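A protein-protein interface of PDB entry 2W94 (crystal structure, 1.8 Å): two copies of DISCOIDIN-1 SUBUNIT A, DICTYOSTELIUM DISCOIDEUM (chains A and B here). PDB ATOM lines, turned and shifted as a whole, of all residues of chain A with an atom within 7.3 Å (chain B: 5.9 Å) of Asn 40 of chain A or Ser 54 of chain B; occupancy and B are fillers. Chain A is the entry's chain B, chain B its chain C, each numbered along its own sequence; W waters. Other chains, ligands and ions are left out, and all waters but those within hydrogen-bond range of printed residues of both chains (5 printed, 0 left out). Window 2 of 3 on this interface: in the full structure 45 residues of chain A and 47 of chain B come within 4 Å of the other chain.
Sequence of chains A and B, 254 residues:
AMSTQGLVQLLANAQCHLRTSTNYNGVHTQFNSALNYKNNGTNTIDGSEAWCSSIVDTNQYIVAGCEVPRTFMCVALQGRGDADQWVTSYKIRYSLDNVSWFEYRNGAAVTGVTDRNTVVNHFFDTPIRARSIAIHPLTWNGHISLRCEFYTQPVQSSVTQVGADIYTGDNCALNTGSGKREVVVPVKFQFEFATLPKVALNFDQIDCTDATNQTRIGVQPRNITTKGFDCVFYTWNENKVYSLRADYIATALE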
ATOM      1  N   TYR A  37      21.130   5.628  12.166  1.00  0.00           N
ATOM      2  CA  TYR A  37      19.801   6.194  12.142  1.00  0.00           C
ATOM      3  C   TYR A  37      19.182   6.043  10.748  1.00  0.00           C
ATOM      4  O   TYR A  37      19.822   6.289   9.757  1.00  0.00           O
ATOM      5  CB  TYR A  37      19.787   7.658  12.580  1.00  0.00           C
ATOM      6  CG  TYR A  37      18.483   8.381  12.294  1.00  0.00           C
ATOM      7  CD1 TYR A  37      18.325   9.093  11.131  1.00  0.00           C
ATOM      8  CD2 TYR A  37      17.444   8.410  13.209  1.00  0.00           C
ATOM      9  CE1 TYR A  37      17.185   9.808  10.866  1.00  0.00           C
ATOM     10  CE2 TYR A  37      16.219   9.135  12.927  1.00  0.00           C
ATOM     11  CZ  TYR A  37      16.115   9.788  11.739  1.00  0.00           C
ATOM     12  OH  TYR A  37      14.986  10.491  11.368  1.00  0.00           O
ATOM     13  N   LYS A  38      17.940   5.584  10.720  1.00  0.00           N
ATOM     14  CA  LYS A  38      17.156   5.446   9.460  1.00  0.00           C
ATOM     15  C   LYS A  38      15.733   5.963   9.644  1.00  0.00           C
ATOM     16  O   LYS A  38      15.132   5.777  10.660  1.00  0.00           O
ATOM     17  CB  LYS A  38      17.128   3.985   8.982  1.00  0.00           C
ATOM     18  CG  LYS A  38      18.545   3.480   8.625  1.00  0.00           C
ATOM     19  CD  LYS A  38      18.523   2.076   8.065  1.00  0.00           C
ATOM     20  CE  LYS A  38      17.852   1.085   8.999  1.00  0.00           C
ATOM     21  NZ  LYS A  38      17.780  -0.307   8.397  1.00  0.00           N
ATOM     22  N   ASN A  39      15.203   6.631   8.625  1.00  0.00           N
ATOM     23  CA  ASN A  39      13.892   7.216   8.706  1.00  0.00           C
ATOM     24  C   ASN A  39      13.007   6.639   7.601  1.00  0.00           C
ATOM     25  O   ASN A  39      13.311   5.602   7.022  1.00  0.00           O
ATOM     26  CB  ASN A  39      13.939   8.778   8.658  1.00  0.00           C
ATOM     27  CG  ASN A  39      14.571   9.356   7.392  1.00  0.00           C
ATOM     28  OD1 ASN A  39      14.733   8.698   6.351  1.00  0.00           O
ATOM     29  ND2 ASN A  39      14.913  10.637   7.470  1.00  0.00           N
ATOM     30  N   ASN A  40      11.899   7.317   7.353  1.00  0.00           N
ATOM     31  CA  ASN A  40      10.934   6.901   6.382  1.00  0.00           C
ATOM     32  C   ASN A  40      11.439   7.354   5.008  1.00  0.00           C
ATOM     33  O   ASN A  40      11.477   8.541   4.666  1.00  0.00           O
ATOM     34  CB  ASN A  40       9.567   7.502   6.756  1.00  0.00           C
ATOM     35  CG  ASN A  40       8.461   6.996   5.911  1.00  0.00           C
ATOM     36  OD1 ASN A  40       8.669   6.666   4.763  1.00  0.00           O
ATOM     37  ND2 ASN A  40       7.269   6.911   6.481  1.00  0.00           N
ATOM     38  N   GLY A  41      11.920   6.402   4.226  1.00  0.00           N
ATOM     39  CA  GLY A  41      12.366   6.725   2.888  1.00  0.00           C
ATOM     40  C   GLY A  41      11.273   6.938   1.835  1.00  0.00           C
ATOM     41  O   GLY A  41      11.585   7.250   0.707  1.00  0.00           O
ATOM     42  N   THR A  42      10.016   6.730   2.154  1.00  0.00           N
ATOM     43  CA  THR A  42       8.951   7.029   1.191  1.00  0.00           C
ATOM     44  C   THR A  42       8.329   8.419   1.428  1.00  0.00           C
ATOM     45  O   THR A  42       7.575   8.933   0.601  1.00  0.00           O
ATOM     46  CB  THR A  42       7.836   6.032   1.237  1.00  0.00           C
ATOM     47  OG1 THR A  42       7.057   6.210   2.436  1.00  0.00           O
ATOM     48  CG2 THR A  42       8.380   4.654   1.226  1.00  0.00           C
ATOM     49  N   ASN A  43       8.656   9.030   2.541  1.00  0.00           N
ATOM     50  CA  ASN A  43       8.126  10.356   2.855  1.00  0.00           C
ATOM     51  C   ASN A  43       9.327  11.282   3.019  1.00  0.00           C
ATOM     52  O   ASN A  43      10.199  11.002   3.824  1.00  0.00           O
ATOM     53  CB  ASN A  43       7.376  10.209   4.169  1.00  0.00           C
ATOM     54  CG  ASN A  43       6.415  11.329   4.459  1.00  0.00           C
ATOM     55  OD1 ASN A  43       5.537  11.173   5.328  1.00  0.00           O
ATOM     56  ND2 ASN A  43       6.573  12.460   3.785  1.00  0.00           N
ATOM     57  N   THR A  44       9.314  12.437   2.349  1.00  0.00           N
ATOM     58  CA  THR A  44      10.405  13.384   2.426  1.00  0.00           C
ATOM     59  C   THR A  44      10.344  14.294   3.665  1.00  0.00           C
ATOM     60  O   THR A  44      11.355  14.930   3.995  1.00  0.00           O
ATOM     61  CB  THR A  44      10.422  14.344   1.156  1.00  0.00           C
ATOM     62  OG1 THR A  44       9.161  15.007   1.053  1.00  0.00           O
ATOM     63  CG2 THR A  44      10.694  13.555  -0.118  1.00  0.00           C
ATOM     64  N   ILE A  45       9.199  14.378   4.321  1.00  0.00           N
ATOM     65  CA  ILE A  45       8.999  15.399   5.317  1.00  0.00           C
ATOM     66  C   ILE A  45       9.781  15.177   6.596  1.00  0.00           C
ATOM     67  O   ILE A  45       9.938  16.123   7.377  1.00  0.00           O
ATOM     68  CB  ILE A  45       7.511  15.592   5.718  1.00  0.00           C
ATOM     69  CG1 ILE A  45       7.006  14.423   6.511  1.00  0.00           C
ATOM     70  CG2 ILE A  45       6.657  15.803   4.481  1.00  0.00           C
ATOM     71  CD1 ILE A  45       5.647  14.663   7.033  1.00  0.00           C
ATOM     72  N   ASP A  46      10.230  13.952   6.847  1.00  0.00           N
ATOM     73  CA  ASP A  46      11.027  13.704   8.074  1.00  0.00           C
ATOM     74  C   ASP A  46      12.522  13.898   7.871  1.00  0.00           C
ATOM     75  O   ASP A  46      13.289  13.652   8.800  1.00  0.00           O
ATOM     76  CB  ASP A  46      10.720  12.326   8.693  1.00  0.00           C
ATOM     77  CG  ASP A  46      11.051  11.184   7.777  1.00  0.00           C
ATOM     78  OD1 ASP A  46      11.250  11.373   6.556  1.00  0.00           O
ATOM     79  OD2 ASP A  46      11.115  10.023   8.288  1.00  0.00           O
ATOM     80  N   GLY A  47      12.935  14.355   6.679  1.00  0.00           N
ATOM     81  CA  GLY A  47      14.264  14.873   6.471  1.00  0.00           C
ATOM     82  C   GLY A  47      15.381  13.854   6.327  1.00  0.00           C
ATOM     83  O   GLY A  47      15.172  12.757   5.772  1.00  0.00           O
ATOM     84  N   GLU A  49      18.809  11.344   6.968  1.00  0.00           N
ATOM     85  CA  GLU A  49      19.413  10.330   7.834  1.00  0.00           C
ATOM     86  C   GLU A  49      20.859  10.786   8.235  1.00  0.00           C
ATOM     87  O   GLU A  49      21.847  10.156   7.892  1.00  0.00           O
ATOM     88  CB  GLU A  49      19.415   8.980   7.121  1.00  0.00           C
ATOM     89  CG  GLU A  49      18.012   8.428   6.937  1.00  0.00           C
ATOM     90  CD  GLU A  49      18.009   7.091   6.136  1.00  0.00           C
ATOM     91  OE1 GLU A  49      18.935   6.862   5.323  1.00  0.00           O
ATOM     92  OE2 GLU A  49      17.078   6.315   6.349  1.00  0.00           O
ATOM     93  N   THR B  22      12.096   7.700  15.191  1.00  0.00           N
ATOM     94  CA  THR B  22      11.823   8.604  14.057  1.00  0.00           C
ATOM     95  C   THR B  22      10.853   9.634  14.563  1.00  0.00           C
ATOM     96  O   THR B  22      10.151   9.392  15.524  1.00  0.00           O
ATOM     97  CB  THR B  22      11.166   7.878  12.814  1.00  0.00           C
ATOM     98  OG1 THR B  22       9.917   7.270  13.209  1.00  0.00           O
ATOM     99  CG2 THR B  22      12.070   6.868  12.188  1.00  0.00           C
ATOM    100  N   ASN B  23      10.812  10.784  13.893  1.00  0.00           N
ATOM    101  CA  ASN B  23       9.911  11.902  14.178  1.00  0.00           C
ATOM    102  C   ASN B  23       9.155  12.282  12.888  1.00  0.00           C
ATOM    103  O   ASN B  23       9.774  12.403  11.833  1.00  0.00           O
ATOM    104  CB  ASN B  23      10.709  13.122  14.622  1.00  0.00           C
ATOM    105  CG  ASN B  23      11.386  12.937  15.991  1.00  0.00           C
ATOM    106  OD1 ASN B  23      10.845  12.304  16.886  1.00  0.00           O
ATOM    107  ND2 ASN B  23      12.518  13.602  16.170  1.00  0.00           N
ATOM    108  N   TYR B  24       7.830  12.405  12.981  1.00  0.00           N
ATOM    109  CA  TYR B  24       6.963  12.636  11.801  1.00  0.00           C
ATOM    110  C   TYR B  24       7.492  13.825  10.991  1.00  0.00           C
ATOM    111  O   TYR B  24       7.667  13.740   9.777  1.00  0.00           O
ATOM    112  CB  TYR B  24       5.533  12.870  12.258  1.00  0.00           C
ATOM    113  CG  TYR B  24       4.523  12.988  11.142  1.00  0.00           C
ATOM    114  CD1 TYR B  24       4.145  11.903  10.419  1.00  0.00           C
ATOM    115  CD2 TYR B  24       3.949  14.214  10.846  1.00  0.00           C
ATOM    116  CE1 TYR B  24       3.216  12.009   9.392  1.00  0.00           C
ATOM    117  CE2 TYR B  24       3.021  14.338   9.853  1.00  0.00           C
ATOM    118  CZ  TYR B  24       2.674  13.237   9.114  1.00  0.00           C
ATOM    119  OH  TYR B  24       1.742  13.352   8.109  1.00  0.00           O
ATOM    120  N   ASN B  25       7.792  14.907  11.694  1.00  0.00           N
ATOM    121  CA  ASN B  25       8.620  15.986  11.187  1.00  0.00           C
ATOM    122  C   ASN B  25       9.158  16.769  12.366  1.00  0.00           C
ATOM    123  O   ASN B  25       9.075  16.262  13.488  1.00  0.00           O
ATOM    124  CB  ASN B  25       7.907  16.860  10.134  1.00  0.00           C
ATOM    125  CG  ASN B  25       6.809  17.743  10.697  1.00  0.00           C
ATOM    126  OD1 ASN B  25       6.656  17.898  11.904  1.00  0.00           O
ATOM    127  ND2 ASN B  25       6.097  18.449   9.778  1.00  0.00           N
ATOM    128  N   CYS B  52       5.267  12.061  17.788  1.00  0.00           N
ATOM    129  CA  CYS B  52       4.692  11.170  16.763  1.00  0.00           C
ATOM    130  C   CYS B  52       5.750  10.655  15.826  1.00  0.00           C
ATOM    131  O   CYS B  52       6.544  11.415  15.352  1.00  0.00           O
ATOM    132  CB  CYS B  52       3.617  11.881  15.938  1.00  0.00           C
ATOM    133  SG  CYS B  52       2.291  12.806  16.823  1.00  0.00           S
ATOM    134  N   SER B  53       5.745   9.340  15.565  1.00  0.00           N
ATOM    135  CA  SER B  53       6.709   8.701  14.704  1.00  0.00           C
ATOM    136  C   SER B  53       6.499   8.990  13.227  1.00  0.00           C
ATOM    137  O   SER B  53       5.414   9.396  12.834  1.00  0.00           O
ATOM    138  CB  SER B  53       6.696   7.181  14.901  1.00  0.00           C
ATOM    139  OG  SER B  53       5.506   6.597  14.397  1.00  0.00           O
ATOM    140  N   SER B  54       7.549   8.821  12.427  1.00  0.00           N
ATOM    141  CA  SER B  54       7.464   8.915  10.966  1.00  0.00           C
ATOM    142  C   SER B  54       7.076   7.564  10.381  1.00  0.00           C
ATOM    143  O   SER B  54       6.326   7.463   9.437  1.00  0.00           O
ATOM    144  CB  SER B  54       8.811   9.329  10.364  1.00  0.00           C
ATOM    145  OG  SER B  54       8.653   9.568   8.981  1.00  0.00           O
ATOM    146  N   ILE B  55       7.622   6.504  10.944  1.00  0.00           N
ATOM    147  CA  ILE B  55       7.334   5.156  10.442  1.00  0.00           C
ATOM    148  C   ILE B  55       6.314   4.575  11.398  1.00  0.00           C
ATOM    149  O   ILE B  55       6.417   4.734  12.621  1.00  0.00           O
ATOM    150  CB  ILE B  55       8.565   4.305  10.402  1.00  0.00           C
ATOM    151  CG1 ILE B  55       9.577   4.857   9.360  1.00  0.00           C
ATOM    152  CG2 ILE B  55       8.230   2.819  10.142  1.00  0.00           C
ATOM    153  CD1 ILE B  55      10.901   4.248   9.466  1.00  0.00           C
ATOM    154  N   VAL B  56       5.314   3.923  10.823  1.00  0.00           N
ATOM    155  CA  VAL B  56       4.267   3.324  11.624  1.00  0.00           C
ATOM    156  C   VAL B  56       4.420   1.810  11.537  1.00  0.00           C
ATOM    157  O   VAL B  56       4.034   1.177  10.560  1.00  0.00           O
ATOM    158  CB  VAL B  56       2.901   3.783  11.150  1.00  0.00           C
ATOM    159  CG1 VAL B  56       1.763   3.101  11.937  1.00  0.00           C
ATOM    160  CG2 VAL B  56       2.798   5.264  11.298  1.00  0.00           C
ATOM    161  N   GLN B  60       9.114   1.190  16.672  1.00  0.00           N
ATOM    162  CA  GLN B  60       9.359   2.537  17.112  1.00  0.00           C
ATOM    163  C   GLN B  60       9.580   2.574  18.624  1.00  0.00           C
ATOM    164  O   GLN B  60       9.200   1.658  19.369  1.00  0.00           O
ATOM    165  CB  GLN B  60       8.204   3.450  16.763  1.00  0.00           C
ATOM    166  CG  GLN B  60       7.866   3.551  15.281  1.00  0.00           C
ATOM    167  CD  GLN B  60       9.061   3.867  14.455  1.00  0.00           C
ATOM    168  OE1 GLN B  60       9.604   4.977  14.508  1.00  0.00           O
ATOM    169  NE2 GLN B  60       9.501   2.890  13.675  1.00  0.00           N
ATOM    170  N   HIS B 143      -2.413   6.618  15.000  1.00  0.00           N
ATOM    171  CA  HIS B 143      -1.007   6.794  14.700  1.00  0.00           C
ATOM    172  C   HIS B 143      -0.237   6.490  16.004  1.00  0.00           C
ATOM    173  O   HIS B 143      -0.815   6.499  17.077  1.00  0.00           O
ATOM    174  CB  HIS B 143      -0.747   8.226  14.179  1.00  0.00           C
ATOM    175  CG  HIS B 143       0.616   8.430  13.551  1.00  0.00           C
ATOM    176  ND1 HIS B 143       0.861   8.244  12.209  1.00  0.00           N
ATOM    177  CD2 HIS B 143       1.791   8.837  14.091  1.00  0.00           C
ATOM    178  CE1 HIS B 143       2.125   8.522  11.944  1.00  0.00           C
ATOM    179  NE2 HIS B 143       2.720   8.866  13.083  1.00  0.00           N
HETATM  180  O   HOH W   1      12.308  10.418  11.198  1.00  0.00           O
HETATM  181  O   HOH W   2       4.973   9.177   7.720  1.00  0.00           O
HETATM  182  O   HOH W   3      13.819  11.677  13.444  1.00  0.00           O
HETATM  183  O   HOH W   4      12.128  14.181  11.382  1.00  0.00           O
HETATM  184  O   HOH W   5       6.909  11.592   8.311  1.00  0.00           O
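O of Ser 54 of chain B lies within hydrogen-bond range of ND2 of Asn 40 of chain A (3.2 Å).
OG of Ser 54 of chain B is in hydrogen-bond range of OD2 of Asp 46 of chain A (2.6 Å).
The backbone NH of Asn 39 of chain A lies within hydrogen-bond range of the side-chain carboxylate of Glu 49 of chain A (3.0 Å).
The backbone NH (N) of Tyr 24 of chain B sits at hydrogen-bond distance from the backbone carbonyl oxygen (O) of Cys 52 of chain B (2.9 Å).
The side-chain hydroxyl (OG) of Ser 53 of chain B lies within hydrogen-bond range of the backbone carbonyl oxygen (O) of Ile 55 of chain B (2.7 Å).
The backbone NH of Ser 54 of chain B lies within hydrogen-bond range of the side-chain hydroxyl of Thr 22 of chain B.
ND2 of Asn 39 of chain A lies within hydrogen-bond range of O of Gly 47 of chain A, at 2.7 Å.
The side-chain amide nitrogen of Asn 43 of chain A sits close to the backbone NH of Ile 45 of chain A.
Lys 38 of chain A touches Thr 22 of chain B (O to CG2, 3.6 Å).
CA of Asn 39 of chain A touches CG2 of Thr 22 of chain B, 3.9 Å away.
Asn 39 of chain A touches Ile 55 of chain B.
Asn 40 of chain A touches Ile 55 of chain B (CB to CG1, 3.7 Å).
Ile 45 of chain A touches Tyr 24 of chain B (CG1 to O, 3.4 Å).
O of Ile 45 of chain A touches CB of Asn 25 of chain B, at 3.5 Å.
CB of Asp 46 of chain A touches O of Asn 23 of chain B, 3.3 Å away.
O of Tyr 24 of chain B touches CB of Asp 46 of chain A, at 3.5 Å.
Of the printed residues of chain B, Asn 40 of chain A touches Ser 54 (3.2 Å) and Ile 55 (3.7 Å).
Ser 54 of chain B touches just these residues of chain A: Asn 40 and Asp 46.
Of the printed residues of chain B, Lys 38 of chain A touches Thr 22.
Printed residues of chain A within 4 Å of Asn 23 of chain B: Asp 46 (3.3 Å).
Tyr 37 of chain A touches none of the printed residues of chain B.
Glu 49 of chain A touches none of the printed residues of chain B.
The nearest residue of chain B that does not touch Asn 40 of chain A is Thr 22 of chain B (4.9 Å).
The nearest printed residue of chain B that does not touch Lys 38 of chain A is Ile 55 of chain B (4.7 Å).
Hydrophobic or aromatic side chains of chain B within 4 Å of the printed part of chain A: Tyr 24 and Ile 55.
Along chain B the printed residues that touch a printed residue of chain A span positions 22 to 55.
Among the printed residues, 10 pairs touch across the chains.
Among the printed residues, no Asp or Glu carboxylate lies within 4 Å of a Lys or Arg side-chain nitrogen of the other chain.
No position is printed for both chains.
Water W3 lies within hydrogen-bond range of the side-chain hydroxyl (OH) of Tyr 37 of chain A (2.7 Å) and the backbone NH (N) of Asn 23 of chain B (3.2 Å).
Water W1 lies within hydrogen-bond range of the side-chain hydroxyl (OH) of Tyr 37 of chain A, the backbone NH (N) of Asn 23 of chain B and the side-chain carboxylate (OD2) of Asp 46 of chain A.
Water W5 lies within hydrogen-bond range of the backbone carbonyl oxygen (O) of Tyr 24 of chain B, the side-chain hydroxyl (OG) of Ser 54 of chain B and the side-chain amide oxygen (OD1) of Asn 43 of chain A.
Water W2 lies within hydrogen-bond range of O of Ser 54 of chain B, OD1 of Asn 43 of chain A and ND2 of Asn 40 of chain A.
Water W4 bridges the backbone carbonyl oxygen (O) of Asp 46 of chain A (2.9 Å) and the backbone carbonyl oxygen (O) of Asn 23 of chain B (3.0 Å).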
